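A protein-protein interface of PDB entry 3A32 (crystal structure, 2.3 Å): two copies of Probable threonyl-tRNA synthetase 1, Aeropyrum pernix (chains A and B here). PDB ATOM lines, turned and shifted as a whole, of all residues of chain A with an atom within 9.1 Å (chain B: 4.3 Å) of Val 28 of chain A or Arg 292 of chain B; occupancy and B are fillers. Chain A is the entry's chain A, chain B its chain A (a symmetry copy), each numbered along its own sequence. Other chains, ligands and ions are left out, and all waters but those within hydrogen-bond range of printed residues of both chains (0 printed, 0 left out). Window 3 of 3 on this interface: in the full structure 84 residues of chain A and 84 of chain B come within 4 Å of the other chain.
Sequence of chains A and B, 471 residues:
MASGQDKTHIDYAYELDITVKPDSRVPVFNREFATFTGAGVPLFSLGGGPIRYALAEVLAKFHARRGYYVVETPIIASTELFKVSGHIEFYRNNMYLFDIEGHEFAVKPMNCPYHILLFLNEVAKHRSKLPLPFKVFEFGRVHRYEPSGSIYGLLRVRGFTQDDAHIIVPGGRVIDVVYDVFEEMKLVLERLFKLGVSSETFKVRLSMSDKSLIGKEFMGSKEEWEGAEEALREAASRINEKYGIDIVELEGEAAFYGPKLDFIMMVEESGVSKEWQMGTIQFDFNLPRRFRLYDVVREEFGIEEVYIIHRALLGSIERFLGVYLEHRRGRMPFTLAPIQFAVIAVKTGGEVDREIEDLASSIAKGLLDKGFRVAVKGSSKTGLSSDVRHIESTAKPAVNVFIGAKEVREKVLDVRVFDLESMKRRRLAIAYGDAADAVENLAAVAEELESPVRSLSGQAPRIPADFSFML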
ATOM      1  N   ARG A  25      -1.153  -3.527  19.047  1.00  0.00           N
ATOM      2  CA  ARG A  25       0.076  -4.172  18.568  1.00  0.00           C
ATOM      3  C   ARG A  25       1.120  -4.352  19.670  1.00  0.00           C
ATOM      4  O   ARG A  25       1.424  -3.401  20.411  1.00  0.00           O
ATOM      5  CB  ARG A  25       0.694  -3.379  17.397  1.00  0.00           C
ATOM      6  CG  ARG A  25      -0.236  -3.285  16.201  1.00  0.00           C
ATOM      7  CD  ARG A  25      -0.335  -4.564  15.382  1.00  0.00           C
ATOM      8  NE  ARG A  25      -0.941  -4.271  14.086  1.00  0.00           N
ATOM      9  CZ  ARG A  25      -0.881  -5.050  12.999  1.00  0.00           C
ATOM     10  NH1 ARG A  25      -0.222  -6.217  13.015  1.00  0.00           N
ATOM     11  NH2 ARG A  25      -1.481  -4.643  11.872  1.00  0.00           N
ATOM     12  N   VAL A  26       1.667  -5.560  19.768  1.00  0.00           N
ATOM     13  CA  VAL A  26       2.769  -5.816  20.714  1.00  0.00           C
ATOM     14  C   VAL A  26       4.043  -5.077  20.266  1.00  0.00           C
ATOM     15  O   VAL A  26       4.468  -5.251  19.146  1.00  0.00           O
ATOM     16  CB  VAL A  26       3.037  -7.331  20.889  1.00  0.00           C
ATOM     17  CG1 VAL A  26       4.156  -7.573  21.893  1.00  0.00           C
ATOM     18  CG2 VAL A  26       1.760  -8.034  21.360  1.00  0.00           C
ATOM     19  N   PRO A  27       4.634  -4.218  21.127  1.00  0.00           N
ATOM     20  CA  PRO A  27       5.934  -3.579  20.784  1.00  0.00           C
ATOM     21  C   PRO A  27       6.964  -4.545  20.168  1.00  0.00           C
ATOM     22  O   PRO A  27       7.106  -5.672  20.641  1.00  0.00           O
ATOM     23  CB  PRO A  27       6.448  -3.097  22.132  1.00  0.00           C
ATOM     24  CG  PRO A  27       5.239  -2.814  22.939  1.00  0.00           C
ATOM     25  CD  PRO A  27       4.134  -3.766  22.443  1.00  0.00           C
ATOM     26  N   VAL A  28       7.676  -4.107  19.125  1.00  0.00           N
ATOM     27  CA  VAL A  28       8.723  -4.926  18.429  1.00  0.00           C
ATOM     28  C   VAL A  28       8.155  -6.134  17.626  1.00  0.00           C
ATOM     29  O   VAL A  28       8.444  -6.274  16.440  1.00  0.00           O
ATOM     30  CB  VAL A  28       9.967  -5.361  19.343  1.00  0.00           C
ATOM     31  CG1 VAL A  28      11.083  -5.978  18.488  1.00  0.00           C
ATOM     32  CG2 VAL A  28      10.553  -4.183  20.130  1.00  0.00           C
ATOM     33  N   PHE A  29       7.324  -6.986  18.206  1.00  0.00           N
ATOM     34  CA  PHE A  29       6.674  -8.000  17.358  1.00  0.00           C
ATOM     35  C   PHE A  29       5.737  -7.440  16.276  1.00  0.00           C
ATOM     36  O   PHE A  29       5.424  -8.133  15.294  1.00  0.00           O
ATOM     37  CB  PHE A  29       5.897  -8.986  18.199  1.00  0.00           C
ATOM     38  CG  PHE A  29       6.751  -9.828  19.047  1.00  0.00           C
ATOM     39  CD1 PHE A  29       7.281 -11.009  18.553  1.00  0.00           C
ATOM     40  CD2 PHE A  29       7.065  -9.435  20.336  1.00  0.00           C
ATOM     41  CE1 PHE A  29       8.107 -11.809  19.354  1.00  0.00           C
ATOM     42  CE2 PHE A  29       7.878 -10.229  21.135  1.00  0.00           C
ATOM     43  CZ  PHE A  29       8.397 -11.421  20.645  1.00  0.00           C
ATOM     44  N   ASN A  30       5.267  -6.207  16.479  1.00  0.00           N
ATOM     45  CA  ASN A  30       4.170  -5.644  15.679  1.00  0.00           C
ATOM     46  C   ASN A  30       3.156  -6.737  15.173  1.00  0.00           C
ATOM     47  O   ASN A  30       2.843  -6.859  13.985  1.00  0.00           O
ATOM     48  CB  ASN A  30       4.738  -4.712  14.578  1.00  0.00           C
ATOM     49  CG  ASN A  30       3.661  -3.844  13.881  1.00  0.00           C
ATOM     50  OD1 ASN A  30       2.564  -3.601  14.414  1.00  0.00           O
ATOM     51  ND2 ASN A  30       3.998  -3.361  12.677  1.00  0.00           N
ATOM     52  N   ARG A  31       2.699  -7.558  16.111  1.00  0.00           N
ATOM     53  CA  ARG A  31       1.551  -8.422  15.933  1.00  0.00           C
ATOM     54  C   ARG A  31       0.565  -7.963  17.009  1.00  0.00           C
ATOM     55  O   ARG A  31       0.960  -7.284  17.981  1.00  0.00           O
ATOM     56  CB  ARG A  31       1.901  -9.887  16.200  1.00  0.00           C
ATOM     57  CG  ARG A  31       2.993 -10.483  15.326  1.00  0.00           C
ATOM     58  CD  ARG A  31       3.414 -11.891  15.880  1.00  0.00           C
ATOM     59  NE  ARG A  31       4.871 -12.198  15.756  1.00  0.00           N
ATOM     60  CZ  ARG A  31       5.491 -13.197  16.404  1.00  0.00           C
ATOM     61  NH1 ARG A  31       4.796 -13.995  17.212  1.00  0.00           N
ATOM     62  NH2 ARG A  31       6.802 -13.410  16.245  1.00  0.00           N
ATOM     63  N   PHE A  33      -2.033  -8.286  20.181  1.00  0.00           N
ATOM     64  CA  PHE A  33      -2.036  -9.077  21.399  1.00  0.00           C
ATOM     65  C   PHE A  33      -2.815 -10.363  21.181  1.00  0.00           C
ATOM     66  O   PHE A  33      -2.374 -11.405  21.650  1.00  0.00           O
ATOM     67  CB  PHE A  33      -2.480  -8.286  22.646  1.00  0.00           C
ATOM     68  CG  PHE A  33      -1.393  -7.386  23.201  1.00  0.00           C
ATOM     69  CD1 PHE A  33      -0.505  -7.849  24.172  1.00  0.00           C
ATOM     70  CD2 PHE A  33      -1.229  -6.074  22.713  1.00  0.00           C
ATOM     71  CE1 PHE A  33       0.524  -7.042  24.647  1.00  0.00           C
ATOM     72  CE2 PHE A  33      -0.211  -5.277  23.165  1.00  0.00           C
ATOM     73  CZ  PHE A  33       0.649  -5.739  24.140  1.00  0.00           C
ATOM     74  N   PHE A  36      -1.393 -13.910  20.346  1.00  0.00           N
ATOM     75  CA  PHE A  36      -0.653 -14.638  21.366  1.00  0.00           C
ATOM     76  C   PHE A  36      -1.661 -15.244  22.303  1.00  0.00           C
ATOM     77  O   PHE A  36      -1.471 -16.357  22.800  1.00  0.00           O
ATOM     78  CB  PHE A  36       0.176 -13.720  22.212  1.00  0.00           C
ATOM     79  CG  PHE A  36       1.330 -13.099  21.523  1.00  0.00           C
ATOM     80  CD1 PHE A  36       2.583 -13.702  21.561  1.00  0.00           C
ATOM     81  CD2 PHE A  36       1.205 -11.852  20.922  1.00  0.00           C
ATOM     82  CE1 PHE A  36       3.693 -13.079  20.978  1.00  0.00           C
ATOM     83  CE2 PHE A  36       2.290 -11.247  20.302  1.00  0.00           C
ATOM     84  CZ  PHE A  36       3.540 -11.854  20.338  1.00  0.00           C
ATOM     85  N   PRO B 288      13.906 -12.533  28.190  1.00  0.00           N
ATOM     86  CA  PRO B 288      14.227 -11.229  27.585  1.00  0.00           C
ATOM     87  C   PRO B 288      14.716 -11.278  26.135  1.00  0.00           C
ATOM     88  O   PRO B 288      14.633 -10.259  25.417  1.00  0.00           O
ATOM     89  CB  PRO B 288      15.336 -10.664  28.490  1.00  0.00           C
ATOM     90  CG  PRO B 288      15.848 -11.821  29.287  1.00  0.00           C
ATOM     91  CD  PRO B 288      14.745 -12.830  29.370  1.00  0.00           C
ATOM     92  N   ARG B 289      15.253 -12.433  25.724  1.00  0.00           N
ATOM     93  CA  ARG B 289      15.559 -12.705  24.313  1.00  0.00           C
ATOM     94  C   ARG B 289      14.264 -13.044  23.532  1.00  0.00           C
ATOM     95  O   ARG B 289      13.975 -12.433  22.494  1.00  0.00           O
ATOM     96  CB  ARG B 289      16.623 -13.835  24.180  1.00  0.00           C
ATOM     97  CG  ARG B 289      18.081 -13.345  24.456  1.00  0.00           C
ATOM     98  CD  ARG B 289      19.109 -14.508  24.394  1.00  0.00           C
ATOM     99  NE  ARG B 289      20.494 -14.044  24.508  1.00  0.00           N
ATOM    100  CZ  ARG B 289      21.109 -13.776  25.650  1.00  0.00           C
ATOM    101  NH1 ARG B 289      20.471 -13.917  26.817  1.00  0.00           N
ATOM    102  NH2 ARG B 289      22.351 -13.324  25.622  1.00  0.00           N
ATOM    103  N   ARG B 290      13.491 -14.012  24.022  1.00  0.00           N
ATOM    104  CA  ARG B 290      12.303 -14.470  23.299  1.00  0.00           C
ATOM    105  C   ARG B 290      11.210 -13.393  23.118  1.00  0.00           C
ATOM    106  O   ARG B 290      10.564 -13.330  22.065  1.00  0.00           O
ATOM    107  CB  ARG B 290      11.732 -15.723  23.962  1.00  0.00           C
ATOM    108  CG  ARG B 290      12.678 -16.926  23.938  1.00  0.00           C
ATOM    109  CD  ARG B 290      12.964 -17.413  22.531  1.00  0.00           C
ATOM    110  NE  ARG B 290      11.897 -18.264  21.960  1.00  0.00           N
ATOM    111  CZ  ARG B 290      11.623 -18.382  20.641  1.00  0.00           C
ATOM    112  NH1 ARG B 290      12.320 -17.693  19.718  1.00  0.00           N
ATOM    113  NH2 ARG B 290      10.635 -19.171  20.228  1.00  0.00           N
ATOM    114  N   PHE B 291      11.035 -12.541  24.124  1.00  0.00           N
ATOM    115  CA  PHE B 291      10.065 -11.437  24.067  1.00  0.00           C
ATOM    116  C   PHE B 291      10.711 -10.079  23.784  1.00  0.00           C
ATOM    117  O   PHE B 291      10.059  -9.056  23.935  1.00  0.00           O
ATOM    118  CB  PHE B 291       9.313 -11.339  25.394  1.00  0.00           C
ATOM    119  CG  PHE B 291       8.259 -12.399  25.566  1.00  0.00           C
ATOM    120  CD1 PHE B 291       6.986 -12.227  25.019  1.00  0.00           C
ATOM    121  CD2 PHE B 291       8.558 -13.586  26.234  1.00  0.00           C
ATOM    122  CE1 PHE B 291       6.016 -13.200  25.185  1.00  0.00           C
ATOM    123  CE2 PHE B 291       7.600 -14.569  26.390  1.00  0.00           C
ATOM    124  CZ  PHE B 291       6.336 -14.384  25.864  1.00  0.00           C
ATOM    125  N   ARG B 292      12.000 -10.080  23.427  1.00  0.00           N
ATOM    126  CA  ARG B 292      12.704  -8.904  22.978  1.00  0.00           C
ATOM    127  C   ARG B 292      12.695  -7.801  24.028  1.00  0.00           C
ATOM    128  O   ARG B 292      12.585  -6.609  23.699  1.00  0.00           O
ATOM    129  CB  ARG B 292      12.158  -8.466  21.608  1.00  0.00           C
ATOM    130  CG  ARG B 292      12.468  -9.536  20.534  1.00  0.00           C
ATOM    131  CD  ARG B 292      11.420  -9.522  19.436  1.00  0.00           C
ATOM    132  NE  ARG B 292      11.513 -10.624  18.455  1.00  0.00           N
ATOM    133  CZ  ARG B 292      10.849 -10.639  17.297  1.00  0.00           C
ATOM    134  NH1 ARG B 292      10.072  -9.618  16.961  1.00  0.00           N
ATOM    135  NH2 ARG B 292      10.961 -11.664  16.461  1.00  0.00           N
ATOM    136  N   LEU B 293      12.879  -8.201  25.290  1.00  0.00           N
ATOM    137  CA  LEU B 293      12.853  -7.267  26.417  1.00  0.00           C
ATOM    138  C   LEU B 293      14.100  -6.421  26.544  1.00  0.00           C
ATOM    139  O   LEU B 293      14.027  -5.273  26.999  1.00  0.00           O
ATOM    140  CB  LEU B 293      12.569  -7.998  27.734  1.00  0.00           C
ATOM    141  CG  LEU B 293      11.264  -8.845  27.746  1.00  0.00           C
ATOM    142  CD1 LEU B 293      11.007  -9.391  29.131  1.00  0.00           C
ATOM    143  CD2 LEU B 293      10.046  -7.989  27.186  1.00  0.00           C
ATOM    144  N   TYR B 294      15.236  -7.015  26.177  1.00  0.00           N
ATOM    145  CA  TYR B 294      16.526  -6.333  26.160  1.00  0.00           C
ATOM    146  C   TYR B 294      16.481  -5.150  25.142  1.00  0.00           C
ATOM    147  O   TYR B 294      16.922  -4.070  25.451  1.00  0.00           O
ATOM    148  CB  TYR B 294      17.651  -7.306  25.800  1.00  0.00           C
ATOM    149  CG  TYR B 294      18.085  -8.296  26.865  1.00  0.00           C
ATOM    150  CD1 TYR B 294      18.075  -7.959  28.212  1.00  0.00           C
ATOM    151  CD2 TYR B 294      18.524  -9.575  26.512  1.00  0.00           C
ATOM    152  CE1 TYR B 294      18.475  -8.846  29.173  1.00  0.00           C
ATOM    153  CE2 TYR B 294      18.948 -10.475  27.470  1.00  0.00           C
ATOM    154  CZ  TYR B 294      18.918 -10.104  28.801  1.00  0.00           C
ATOM    155  OH  TYR B 294      19.360 -10.956  29.797  1.00  0.00           O
ATOM    156  N   ASP B 295      15.927  -5.413  23.953  1.00  0.00           N
ATOM    157  CA  ASP B 295      15.651  -4.406  22.926  1.00  0.00           C
ATOM    158  C   ASP B 295      14.705  -3.327  23.426  1.00  0.00           C
ATOM    159  O   ASP B 295      15.060  -2.143  23.415  1.00  0.00           O
ATOM    160  CB  ASP B 295      15.126  -5.068  21.642  1.00  0.00           C
ATOM    161  CG  ASP B 295      16.215  -5.876  20.927  1.00  0.00           C
ATOM    162  OD1 ASP B 295      17.412  -5.554  21.117  1.00  0.00           O
ATOM    163  OD2 ASP B 295      15.886  -6.843  20.199  1.00  0.00           O
ATOM    164  N   VAL B 296      13.536  -3.745  23.914  1.00  0.00           N
ATOM    165  CA  VAL B 296      12.519  -2.837  24.417  1.00  0.00           C
ATOM    166  C   VAL B 296      13.022  -1.938  25.556  1.00  0.00           C
ATOM    167  O   VAL B 296      12.796  -0.729  25.553  1.00  0.00           O
ATOM    168  CB  VAL B 296      11.205  -3.628  24.791  1.00  0.00           C
ATOM    169  CG1 VAL B 296      10.363  -2.838  25.757  1.00  0.00           C
ATOM    170  CG2 VAL B 296      10.430  -3.954  23.532  1.00  0.00           C
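CG1 of Val 28 of chain A touches CD of Arg 292 of chain B, at 3.7 Å. Val 28 of chain A touches Val 296 of chain B (CG2 to CG2, 3.4 Å). Arg 290 of chain B touches Phe 29 of chain A (O to CZ, 3.2 Å). Phe 29 of chain A touches Phe 291 of chain B. Arg 292 of chain B touches Phe 29 of chain A (NH1 to CD1, 3.5 Å).
No position is printed for both chains.
Printed residues of chain A that touch a printed residue of chain B: Val 28 and Phe 29. Among the printed residues, 5 pairs touch across the chains. Among the printed residues, no Asp or Glu carboxylate lies within 4 Å of a Lys or Arg side-chain nitrogen of the other chain.
Of chain B, only Arg 292 and Val 296 come within 4 Å of Val 28 of chain A. Printed residues of chain A within 4 Å of Arg 292 of chain B: Val 28 (3.7 Å) and Phe 29 (3.5 Å). Of the printed residues of chain A, Phe 291 of chain B touches Phe 29. Printed residues of chain A within 4 Å of Val 296 of chain B: Val 28 (3.4 Å). Printed residues of chain B within 4 Å of Phe 29 of chain A: Arg 290 (3.2 Å), Phe 291 (3.7 Å) and Arg 292 (3.5 Å). Of the printed residues of chain A, Arg 290 of chain B touches Phe 29 (3.2 Å). The nearest printed residue of chain B that does not touch Val 28 of chain A is Asp 295 of chain B (4.9 Å).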
